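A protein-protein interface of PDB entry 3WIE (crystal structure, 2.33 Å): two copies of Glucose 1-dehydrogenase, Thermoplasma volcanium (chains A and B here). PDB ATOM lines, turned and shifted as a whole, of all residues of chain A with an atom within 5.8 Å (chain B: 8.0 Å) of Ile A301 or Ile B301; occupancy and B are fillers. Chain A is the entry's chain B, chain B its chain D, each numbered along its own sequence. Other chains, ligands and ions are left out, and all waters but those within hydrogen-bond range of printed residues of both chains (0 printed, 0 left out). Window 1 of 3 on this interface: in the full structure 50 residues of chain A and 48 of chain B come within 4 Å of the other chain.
N of Gly B303 sits at hydrogen-bond distance from O of Ile A299 (2.8 Å).
The backbone NH of Ile A301 lies within hydrogen-bond range of the backbone carbonyl oxygen of Ile B301 (2.8 Å).
The backbone carbonyl oxygen (O) of Gly A303 is in hydrogen-bond range of the guanidinium group (NH2) of Arg B174.
The backbone NH of Gly A303 sits at hydrogen-bond distance from the backbone carbonyl oxygen of Ile B299, 2.9 Å away.
O of Thr A300 lies within hydrogen-bond range of N of Val A272 (2.8 Å).
The backbone carbonyl oxygen (O) of Ile A294 lies within hydrogen-bond range of the backbone NH (N) of Ile A299, 3.3 Å away.
NH1 of Arg B174 lies within hydrogen-bond range of O of Ile B299, at 3.5 Å.
O of Gly B270 is in hydrogen-bond range of N of Thr B300 (3.2 Å).
The backbone NH (N) of Val B272 sits at hydrogen-bond distance from the backbone carbonyl oxygen (O) of Thr B300 (2.7 Å).
The backbone NH (N) of Leu B274 sits at hydrogen-bond distance from the backbone carbonyl oxygen (O) of Ala B302 (2.8 Å).
Among the printed residues, pairs that only touch across the chains: Ile A294 with Leu B274, Ile A299 with Ala B302, Thr A300 with Thr B300, Thr A300 with Ile B301, Ile A301 with Thr B300, Ala A302 with Arg B174, Ala A302 with Ile B299, Gly A303 with Ile B294 and Gly A303 with Asn B298.
Of the printed residues of chain B, Ile A294 touches Leu B274 (3.98 Å).
Of the printed residues of chain A, Arg B174 touches Ala A302 and Gly A303.
Printed residues of chain A within 4 Å of Ile B294: Gly A303.
The nearest printed residue of chain B that does not touch Ile A299 is Ile B301 (4.1 Å).
Of the 23 printed residues of chain B, 9 touch a printed residue of chain A.
Of the 13 printed residues of chain A, 6 touch a printed residue of chain B.
Printed residues of chain A that touch a printed residue of chain B: Ile A294, Ile A299, Thr A300, Ile A301, Ala A302 and Gly A303.
Hydrophobic or aromatic side chains of chain A that line the printed part of chain B: Ile A294, Ile A301 and Ala A302.
Among the printed residues, no Asp or Glu carboxylate lies within 4 Å of a Lys or Arg side-chain nitrogen of the other chain.
Ile A294 touches Leu B274, but with the chains exchanged Leu A274 does not touch Ile B294 (4.2 Å).
Ile A299 touches Gly B303, and with the chains exchanged Gly A303 touches Ile B299.
Thr A300 touches its own counterpart, Thr B300.
Gly A303 touches Ile B294, but with the chains exchanged Ile A294 does not touch Gly B303 (4.1 Å).
Positions printed for both chains: 260, 263, 270, 271, 272, 273, 274, 294, 299, 300, 301, 302 and 303.
Of the 13 pairs that touch across the chains among the printed residues, 8 have their exchanged pair printed and touching as well.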
ATOM      1  N   PHE A 260      19.611 -30.234 -15.565  1.00  0.00           N
ATOM      2  CA  PHE A 260      20.717 -31.120 -15.929  1.00  0.00           C
ATOM      3  C   PHE A 260      20.717 -31.500 -17.399  1.00  0.00           C
ATOM      4  O   PHE A 260      21.793 -31.536 -18.016  1.00  0.00           O
ATOM      5  CB  PHE A 260      20.868 -32.251 -14.953  1.00  0.00           C
ATOM      6  CG  PHE A 260      21.504 -31.826 -13.679  1.00  0.00           C
ATOM      7  CD1 PHE A 260      22.861 -31.557 -13.632  1.00  0.00           C
ATOM      8  CD2 PHE A 260      20.765 -31.599 -12.569  1.00  0.00           C
ATOM      9  CE1 PHE A 260      23.479 -31.149 -12.451  1.00  0.00           C
ATOM     10  CE2 PHE A 260      21.356 -31.192 -11.389  1.00  0.00           C
ATOM     11  CZ  PHE A 260      22.716 -30.966 -11.335  1.00  0.00           C
ATOM     12  N   VAL A 263      22.248 -28.517 -18.980  1.00  0.00           N
ATOM     13  CA  VAL A 263      23.675 -28.478 -18.677  1.00  0.00           C
ATOM     14  C   VAL A 263      24.455 -29.303 -19.741  1.00  0.00           C
ATOM     15  O   VAL A 263      25.552 -28.876 -20.210  1.00  0.00           O
ATOM     16  CB  VAL A 263      23.942 -28.959 -17.240  1.00  0.00           C
ATOM     17  CG1 VAL A 263      25.390 -29.250 -16.994  1.00  0.00           C
ATOM     18  CG2 VAL A 263      23.533 -27.908 -16.220  1.00  0.00           C
ATOM     19  N   GLY A 270      31.523 -22.636 -20.386  1.00  0.00           N
ATOM     20  CA  GLY A 270      30.176 -22.170 -20.275  1.00  0.00           C
ATOM     21  C   GLY A 270      29.785 -21.893 -18.847  1.00  0.00           C
ATOM     22  O   GLY A 270      30.337 -22.475 -17.922  1.00  0.00           O
ATOM     23  N   VAL A 271      28.788 -21.035 -18.653  1.00  0.00           N
ATOM     24  CA  VAL A 271      28.307 -20.780 -17.276  1.00  0.00           C
ATOM     25  C   VAL A 271      26.843 -21.046 -17.081  1.00  0.00           C
ATOM     26  O   VAL A 271      25.985 -20.639 -17.886  1.00  0.00           O
ATOM     27  CB  VAL A 271      28.565 -19.300 -16.948  1.00  0.00           C
ATOM     28  CG1 VAL A 271      28.076 -18.920 -15.542  1.00  0.00           C
ATOM     29  CG2 VAL A 271      30.014 -19.063 -17.155  1.00  0.00           C
ATOM     30  N   VAL A 272      26.533 -21.603 -15.958  1.00  0.00           N
ATOM     31  CA  VAL A 272      25.178 -21.930 -15.657  1.00  0.00           C
ATOM     32  C   VAL A 272      24.882 -21.139 -14.397  1.00  0.00           C
ATOM     33  O   VAL A 272      25.557 -21.343 -13.399  1.00  0.00           O
ATOM     34  CB  VAL A 272      25.045 -23.431 -15.342  1.00  0.00           C
ATOM     35  CG1 VAL A 272      23.631 -23.812 -14.909  1.00  0.00           C
ATOM     36  CG2 VAL A 272      25.485 -24.233 -16.547  1.00  0.00           C
ATOM     37  N   ILE A 273      23.836 -20.311 -14.424  1.00  0.00           N
ATOM     38  CA  ILE A 273      23.318 -19.666 -13.223  1.00  0.00           C
ATOM     39  C   ILE A 273      22.108 -20.429 -12.692  1.00  0.00           C
ATOM     40  O   ILE A 273      21.108 -20.600 -13.379  1.00  0.00           O
ATOM     41  CB  ILE A 273      22.895 -18.206 -13.475  1.00  0.00           C
ATOM     42  CG1 ILE A 273      24.049 -17.382 -14.025  1.00  0.00           C
ATOM     43  CG2 ILE A 273      22.343 -17.590 -12.197  1.00  0.00           C
ATOM     44  CD1 ILE A 273      25.278 -17.369 -13.129  1.00  0.00           C
ATOM     45  N   LEU A 274      22.189 -20.834 -11.452  1.00  0.00           N
ATOM     46  CA  LEU A 274      21.095 -21.450 -10.774  1.00  0.00           C
ATOM     47  C   LEU A 274      20.419 -20.359  -9.986  1.00  0.00           C
ATOM     48  O   LEU A 274      21.051 -19.635  -9.272  1.00  0.00           O
ATOM     49  CB  LEU A 274      21.581 -22.560  -9.862  1.00  0.00           C
ATOM     50  CG  LEU A 274      22.086 -23.830 -10.519  1.00  0.00           C
ATOM     51  CD1 LEU A 274      22.287 -24.956  -9.547  1.00  0.00           C
ATOM     52  CD2 LEU A 274      21.207 -24.274 -11.651  1.00  0.00           C
ATOM     53  N   ILE A 294      30.950 -31.844 -17.178  1.00  0.00           N
ATOM     54  CA  ILE A 294      31.159 -30.559 -16.496  1.00  0.00           C
ATOM     55  C   ILE A 294      32.652 -30.298 -16.354  1.00  0.00           C
ATOM     56  O   ILE A 294      33.161 -29.268 -16.793  1.00  0.00           O
ATOM     57  CB  ILE A 294      30.420 -30.555 -15.131  1.00  0.00           C
ATOM     58  CG1 ILE A 294      28.911 -30.533 -15.342  1.00  0.00           C
ATOM     59  CG2 ILE A 294      30.801 -29.375 -14.293  1.00  0.00           C
ATOM     60  CD1 ILE A 294      28.125 -30.774 -14.066  1.00  0.00           C
ATOM     61  N   ILE A 299      33.261 -25.993 -17.058  1.00  0.00           N
ATOM     62  CA  ILE A 299      32.012 -25.347 -16.830  1.00  0.00           C
ATOM     63  C   ILE A 299      31.891 -24.905 -15.373  1.00  0.00           C
ATOM     64  O   ILE A 299      32.301 -25.624 -14.468  1.00  0.00           O
ATOM     65  CB  ILE A 299      30.869 -26.268 -17.234  1.00  0.00           C
ATOM     66  CG1 ILE A 299      30.649 -26.119 -18.709  1.00  0.00           C
ATOM     67  CG2 ILE A 299      29.578 -25.947 -16.530  1.00  0.00           C
ATOM     68  CD1 ILE A 299      29.901 -27.302 -19.290  1.00  0.00           C
ATOM     69  N   THR A 300      31.268 -23.740 -15.177  1.00  0.00           N
ATOM     70  CA  THR A 300      30.869 -23.293 -13.849  1.00  0.00           C
ATOM     71  C   THR A 300      29.367 -23.265 -13.639  1.00  0.00           C
ATOM     72  O   THR A 300      28.638 -22.825 -14.480  1.00  0.00           O
ATOM     73  CB  THR A 300      31.408 -21.881 -13.591  1.00  0.00           C
ATOM     74  OG1 THR A 300      32.775 -21.849 -13.955  1.00  0.00           O
ATOM     75  CG2 THR A 300      31.249 -21.490 -12.092  1.00  0.00           C
ATOM     76  N   ILE A 301      28.918 -23.746 -12.493  1.00  0.00           N
ATOM     77  CA  ILE A 301      27.518 -23.735 -12.110  1.00  0.00           C
ATOM     78  C   ILE A 301      27.470 -22.904 -10.836  1.00  0.00           C
ATOM     79  O   ILE A 301      27.976 -23.351  -9.771  1.00  0.00           O
ATOM     80  CB  ILE A 301      27.021 -25.152 -11.810  1.00  0.00           C
ATOM     81  CG1 ILE A 301      27.229 -25.986 -13.068  1.00  0.00           C
ATOM     82  CG2 ILE A 301      25.589 -25.137 -11.323  1.00  0.00           C
ATOM     83  CD1 ILE A 301      26.841 -27.430 -12.987  1.00  0.00           C
ATOM     84  N   ALA A 302      26.884 -21.695 -10.932  1.00  0.00           N
ATOM     85  CA  ALA A 302      26.846 -20.772  -9.785  1.00  0.00           C
ATOM     86  C   ALA A 302      25.416 -20.529  -9.289  1.00  0.00           C
ATOM     87  O   ALA A 302      24.546 -20.073 -10.019  1.00  0.00           O
ATOM     88  CB  ALA A 302      27.559 -19.486 -10.173  1.00  0.00           C
ATOM     89  N   GLY A 303      25.132 -20.868  -8.058  1.00  0.00           N
ATOM     90  CA  GLY A 303      23.876 -20.426  -7.456  1.00  0.00           C
ATOM     91  C   GLY A 303      23.911 -18.958  -7.058  1.00  0.00           C
ATOM     92  O   GLY A 303      24.960 -18.437  -6.677  1.00  0.00           O
ATOM     93  N   VAL B 167      41.297 -21.548 -10.452  1.00  0.00           N
ATOM     94  CA  VAL B 167      39.856 -21.463 -10.661  1.00  0.00           C
ATOM     95  C   VAL B 167      39.145 -21.014  -9.372  1.00  0.00           C
ATOM     96  O   VAL B 167      38.247 -20.181  -9.420  1.00  0.00           O
ATOM     97  CB  VAL B 167      39.259 -22.810 -11.186  1.00  0.00           C
ATOM     98  CG1 VAL B 167      37.760 -22.882 -11.081  1.00  0.00           C
ATOM     99  CG2 VAL B 167      39.730 -23.100 -12.597  1.00  0.00           C
ATOM    100  N   VAL B 171      36.871 -17.586  -8.939  1.00  0.00           N
ATOM    101  CA  VAL B 171      35.471 -17.643  -8.599  1.00  0.00           C
ATOM    102  C   VAL B 171      35.121 -17.211  -7.186  1.00  0.00           C
ATOM    103  O   VAL B 171      34.001 -16.750  -6.932  1.00  0.00           O
ATOM    104  CB  VAL B 171      34.790 -18.996  -8.899  1.00  0.00           C
ATOM    105  CG1 VAL B 171      35.014 -19.391 -10.334  1.00  0.00           C
ATOM    106  CG2 VAL B 171      35.235 -20.083  -7.908  1.00  0.00           C
ATOM    107  N   ARG B 174      33.597 -13.669  -5.955  1.00  0.00           N
ATOM    108  CA  ARG B 174      32.227 -13.236  -6.029  1.00  0.00           C
ATOM    109  C   ARG B 174      31.751 -12.569  -4.719  1.00  0.00           C
ATOM    110  O   ARG B 174      30.813 -11.819  -4.684  1.00  0.00           O
ATOM    111  CB  ARG B 174      31.313 -14.317  -6.587  1.00  0.00           C
ATOM    112  CG  ARG B 174      30.987 -15.475  -5.714  1.00  0.00           C
ATOM    113  CD  ARG B 174      30.168 -16.458  -6.488  1.00  0.00           C
ATOM    114  NE  ARG B 174      28.768 -16.181  -6.325  1.00  0.00           N
ATOM    115  CZ  ARG B 174      27.796 -17.040  -6.440  1.00  0.00           C
ATOM    116  NH1 ARG B 174      28.022 -18.278  -6.753  1.00  0.00           N
ATOM    117  NH2 ARG B 174      26.581 -16.644  -6.234  1.00  0.00           N
ATOM    118  N   LEU B 249      35.254 -27.662  -0.966  1.00  0.00           N
ATOM    119  CA  LEU B 249      35.061 -29.079  -1.216  1.00  0.00           C
ATOM    120  C   LEU B 249      35.663 -29.381  -2.584  1.00  0.00           C
ATOM    121  O   LEU B 249      35.258 -28.786  -3.608  1.00  0.00           O
ATOM    122  CB  LEU B 249      33.560 -29.374  -1.282  1.00  0.00           C
ATOM    123  CG  LEU B 249      33.231 -30.823  -1.617  1.00  0.00           C
ATOM    124  CD1 LEU B 249      33.747 -31.713  -0.473  1.00  0.00           C
ATOM    125  CD2 LEU B 249      31.734 -31.071  -1.882  1.00  0.00           C
ATOM    126  N   ILE B 259      29.676 -36.710  -4.090  1.00  0.00           N
ATOM    127  CA  ILE B 259      29.798 -35.283  -4.411  1.00  0.00           C
ATOM    128  C   ILE B 259      28.643 -34.563  -3.741  1.00  0.00           C
ATOM    129  O   ILE B 259      28.840 -33.664  -2.890  1.00  0.00           O
ATOM    130  CB  ILE B 259      29.801 -35.063  -5.934  1.00  0.00           C
ATOM    131  CG1 ILE B 259      31.111 -35.571  -6.502  1.00  0.00           C
ATOM    132  CG2 ILE B 259      29.676 -33.574  -6.267  1.00  0.00           C
ATOM    133  CD1 ILE B 259      31.074 -35.796  -7.996  1.00  0.00           C
ATOM    134  N   PHE B 260      27.446 -35.014  -4.073  1.00  0.00           N
ATOM    135  CA  PHE B 260      26.220 -34.369  -3.592  1.00  0.00           C
ATOM    136  C   PHE B 260      25.917 -34.486  -2.117  1.00  0.00           C
ATOM    137  O   PHE B 260      25.298 -33.579  -1.563  1.00  0.00           O
ATOM    138  CB  PHE B 260      25.011 -34.716  -4.484  1.00  0.00           C
ATOM    139  CG  PHE B 260      25.061 -34.009  -5.798  1.00  0.00           C
ATOM    140  CD1 PHE B 260      24.774 -32.660  -5.868  1.00  0.00           C
ATOM    141  CD2 PHE B 260      25.524 -34.652  -6.935  1.00  0.00           C
ATOM    142  CE1 PHE B 260      24.887 -31.980  -7.062  1.00  0.00           C
ATOM    143  CE2 PHE B 260      25.650 -33.986  -8.135  1.00  0.00           C
ATOM    144  CZ  PHE B 260      25.328 -32.648  -8.208  1.00  0.00           C
ATOM    145  N   VAL B 263      28.137 -31.825  -0.893  1.00  0.00           N
ATOM    146  CA  VAL B 263      27.672 -30.513  -1.310  1.00  0.00           C
ATOM    147  C   VAL B 263      26.685 -29.974  -0.265  1.00  0.00           C
ATOM    148  O   VAL B 263      26.717 -28.826   0.060  1.00  0.00           O
ATOM    149  CB  VAL B 263      27.101 -30.531  -2.738  1.00  0.00           C
ATOM    150  CG1 VAL B 263      26.240 -29.319  -3.004  1.00  0.00           C
ATOM    151  CG2 VAL B 263      28.210 -30.639  -3.760  1.00  0.00           C
ATOM    152  N   VAL B 266      28.137 -27.750   2.628  1.00  0.00           N
ATOM    153  CA  VAL B 266      28.954 -26.599   2.212  1.00  0.00           C
ATOM    154  C   VAL B 266      28.317 -25.349   2.751  1.00  0.00           C
ATOM    155  O   VAL B 266      27.092 -25.210   2.752  1.00  0.00           O
ATOM    156  CB  VAL B 266      29.103 -26.547   0.690  1.00  0.00           C
ATOM    157  CG1 VAL B 266      29.809 -25.279   0.265  1.00  0.00           C
ATOM    158  CG2 VAL B 266      29.921 -27.764   0.230  1.00  0.00           C
ATOM    159  N   GLY B 270      30.499 -21.065  -0.346  1.00  0.00           N
ATOM    160  CA  GLY B 270      31.410 -22.174  -0.546  1.00  0.00           C
ATOM    161  C   GLY B 270      31.700 -22.415  -1.987  1.00  0.00           C
ATOM    162  O   GLY B 270      30.919 -22.097  -2.842  1.00  0.00           O
ATOM    163  N   VAL B 271      32.863 -22.966  -2.247  1.00  0.00           N
ATOM    164  CA  VAL B 271      33.246 -23.339  -3.587  1.00  0.00           C
ATOM    165  C   VAL B 271      33.454 -24.846  -3.646  1.00  0.00           C
ATOM    166  O   VAL B 271      34.160 -25.441  -2.794  1.00  0.00           O
ATOM    167  CB  VAL B 271      34.544 -22.650  -3.952  1.00  0.00           C
ATOM    168  CG1 VAL B 271      34.998 -23.119  -5.316  1.00  0.00           C
ATOM    169  CG2 VAL B 271      34.384 -21.134  -3.903  1.00  0.00           C
ATOM    170  N   VAL B 272      32.860 -25.466  -4.658  1.00  0.00           N
ATOM    171  CA  VAL B 272      33.014 -26.869  -4.939  1.00  0.00           C
ATOM    172  C   VAL B 272      33.813 -27.032  -6.221  1.00  0.00           C
ATOM    173  O   VAL B 272      33.418 -26.510  -7.259  1.00  0.00           O
ATOM    174  CB  VAL B 272      31.662 -27.524  -5.113  1.00  0.00           C
ATOM    175  CG1 VAL B 272      31.831 -29.032  -5.418  1.00  0.00           C
ATOM    176  CG2 VAL B 272      30.787 -27.309  -3.884  1.00  0.00           C
ATOM    177  N   ILE B 273      34.961 -27.734  -6.158  1.00  0.00           N
ATOM    178  CA  ILE B 273      35.772 -28.027  -7.355  1.00  0.00           C
ATOM    179  C   ILE B 273      35.489 -29.450  -7.798  1.00  0.00           C
ATOM    180  O   ILE B 273      35.666 -30.398  -7.025  1.00  0.00           O
ATOM    181  CB  ILE B 273      37.274 -27.868  -7.079  1.00  0.00           C
ATOM    182  CG1 ILE B 273      37.583 -26.423  -6.601  1.00  0.00           C
ATOM    183  CG2 ILE B 273      38.130 -28.212  -8.316  1.00  0.00           C
ATOM    184  CD1 ILE B 273      37.414 -25.395  -7.714  1.00  0.00           C
ATOM    185  N   LEU B 274      35.085 -29.612  -9.035  1.00  0.00           N
ATOM    186  CA  LEU B 274      34.838 -30.907  -9.580  1.00  0.00           C
ATOM    187  C   LEU B 274      36.041 -31.185 -10.434  1.00  0.00           C
ATOM    188  O   LEU B 274      36.418 -30.397 -11.249  1.00  0.00           O
ATOM    189  CB  LEU B 274      33.547 -30.931 -10.392  1.00  0.00           C
ATOM    190  CG  LEU B 274      32.168 -30.915  -9.746  1.00  0.00           C
ATOM    191  CD1 LEU B 274      31.048 -31.137 -10.736  1.00  0.00           C
ATOM    192  CD2 LEU B 274      32.031 -31.820  -8.557  1.00  0.00           C
ATOM    193  N   ASP B 290      18.044 -29.898  -3.176  1.00  0.00           N
ATOM    194  CA  ASP B 290      19.460 -29.860  -3.417  1.00  0.00           C
ATOM    195  C   ASP B 290      19.806 -28.534  -4.177  1.00  0.00           C
ATOM    196  O   ASP B 290      20.653 -27.758  -3.751  1.00  0.00           O
ATOM    197  CB  ASP B 290      19.883 -31.104  -4.173  1.00  0.00           C
ATOM    198  CG  ASP B 290      19.478 -32.406  -3.438  1.00  0.00           C
ATOM    199  OD1 ASP B 290      19.441 -32.387  -2.185  1.00  0.00           O
ATOM    200  OD2 ASP B 290      19.174 -33.433  -4.105  1.00  0.00           O
ATOM    201  N   ILE B 291      19.060 -28.239  -5.224  1.00  0.00           N
ATOM    202  CA  ILE B 291      19.261 -27.015  -6.001  1.00  0.00           C
ATOM    203  C   ILE B 291      19.148 -25.779  -5.076  1.00  0.00           C
ATOM    204  O   ILE B 291      20.033 -24.918  -5.006  1.00  0.00           O
ATOM    205  CB  ILE B 291      18.230 -26.970  -7.172  1.00  0.00           C
ATOM    206  CG1 ILE B 291      18.407 -28.190  -8.058  1.00  0.00           C
ATOM    207  CG2 ILE B 291      18.318 -25.699  -8.013  1.00  0.00           C
ATOM    208  CD1 ILE B 291      19.840 -28.505  -8.339  1.00  0.00           C
ATOM    209  N   ILE B 294      22.026 -24.914  -2.928  1.00  0.00           N
ATOM    210  CA  ILE B 294      23.048 -24.256  -3.693  1.00  0.00           C
ATOM    211  C   ILE B 294      22.697 -22.825  -3.973  1.00  0.00           C
ATOM    212  O   ILE B 294      23.527 -21.925  -3.786  1.00  0.00           O
ATOM    213  CB  ILE B 294      23.329 -25.033  -4.984  1.00  0.00           C
ATOM    214  CG1 ILE B 294      23.974 -26.374  -4.601  1.00  0.00           C
ATOM    215  CG2 ILE B 294      24.285 -24.327  -5.926  1.00  0.00           C
ATOM    216  CD1 ILE B 294      23.852 -27.415  -5.686  1.00  0.00           C
ATOM    217  N   ASN B 298      24.516 -19.220  -2.323  1.00  0.00           N
ATOM    218  CA  ASN B 298      25.483 -18.663  -3.277  1.00  0.00           C
ATOM    219  C   ASN B 298      26.701 -19.542  -3.453  1.00  0.00           C
ATOM    220  O   ASN B 298      27.808 -19.056  -3.473  1.00  0.00           O
ATOM    221  CB  ASN B 298      26.003 -17.256  -2.856  1.00  0.00           C
ATOM    222  CG  ASN B 298      24.927 -16.135  -2.999  1.00  0.00           C
ATOM    223  OD1 ASN B 298      24.376 -15.848  -4.100  1.00  0.00           O
ATOM    224  ND2 ASN B 298      24.633 -15.507  -1.896  1.00  0.00           N
ATOM    225  N   ILE B 299      26.510 -20.831  -3.559  1.00  0.00           N
ATOM    226  CA  ILE B 299      27.636 -21.751  -3.759  1.00  0.00           C
ATOM    227  C   ILE B 299      27.993 -21.790  -5.242  1.00  0.00           C
ATOM    228  O   ILE B 299      27.150 -21.593  -6.108  1.00  0.00           O
ATOM    229  CB  ILE B 299      27.227 -23.155  -3.255  1.00  0.00           C
ATOM    230  CG1 ILE B 299      27.210 -23.146  -1.731  1.00  0.00           C
ATOM    231  CG2 ILE B 299      28.143 -24.238  -3.828  1.00  0.00           C
ATOM    232  CD1 ILE B 299      26.345 -24.248  -1.157  1.00  0.00           C
ATOM    233  N   THR B 300      29.254 -22.043  -5.521  1.00  0.00           N
ATOM    234  CA  THR B 300      29.762 -22.213  -6.864  1.00  0.00           C
ATOM    235  C   THR B 300      30.383 -23.610  -7.006  1.00  0.00           C
ATOM    236  O   THR B 300      31.161 -24.026  -6.187  1.00  0.00           O
ATOM    237  CB  THR B 300      30.855 -21.181  -7.180  1.00  0.00           C
ATOM    238  OG1 THR B 300      30.359 -19.858  -6.913  1.00  0.00           O
ATOM    239  CG2 THR B 300      31.249 -21.258  -8.674  1.00  0.00           C
ATOM    240  N   ILE B 301      29.985 -24.321  -8.053  1.00  0.00           N
ATOM    241  CA  ILE B 301      30.495 -25.605  -8.409  1.00  0.00           C
ATOM    242  C   ILE B 301      31.256 -25.406  -9.721  1.00  0.00           C
ATOM    243  O   ILE B 301      30.648 -25.101 -10.751  1.00  0.00           O
ATOM    244  CB  ILE B 301      29.358 -26.597  -8.619  1.00  0.00           C
ATOM    245  CG1 ILE B 301      28.506 -26.703  -7.342  1.00  0.00           C
ATOM    246  CG2 ILE B 301      29.961 -27.978  -8.969  1.00  0.00           C
ATOM    247  CD1 ILE B 301      27.252 -27.537  -7.463  1.00  0.00           C
ATOM    248  N   ALA B 302      32.571 -25.569  -9.699  1.00  0.00           N
ATOM    249  CA  ALA B 302      33.373 -25.370 -10.921  1.00  0.00           C
ATOM    250  C   ALA B 302      34.086 -26.621 -11.333  1.00  0.00           C
ATOM    251  O   ALA B 302      34.779 -27.228 -10.538  1.00  0.00           O
ATOM    252  CB  ALA B 302      34.387 -24.298 -10.716  1.00  0.00           C
ATOM    253  N   GLY B 303      33.938 -26.992 -12.598  1.00  0.00           N
ATOM    254  CA  GLY B 303      34.663 -28.143 -13.112  1.00  0.00           C
ATOM    255  C   GLY B 303      35.994 -27.653 -13.575  1.00  0.00           C
ATOM    256  O   GLY B 303      36.050 -26.585 -14.182  1.00  0.00           O
ATOM    257  N   SER B 304      37.065 -28.417 -13.314  1.00  0.00           N
ATOM    258  CA  SER B 304      38.393 -28.037 -13.780  1.00  0.00           C
ATOM    259  C   SER B 304      39.202 -29.171 -14.418  1.00  0.00           C
ATOM    260  O   SER B 304      39.241 -30.243 -13.916  1.00  0.00           O
ATOM    261  CB  SER B 304      39.168 -27.489 -12.617  1.00  0.00           C
ATOM    262  OG  SER B 304      40.419 -26.902 -13.048  1.00  0.00           O
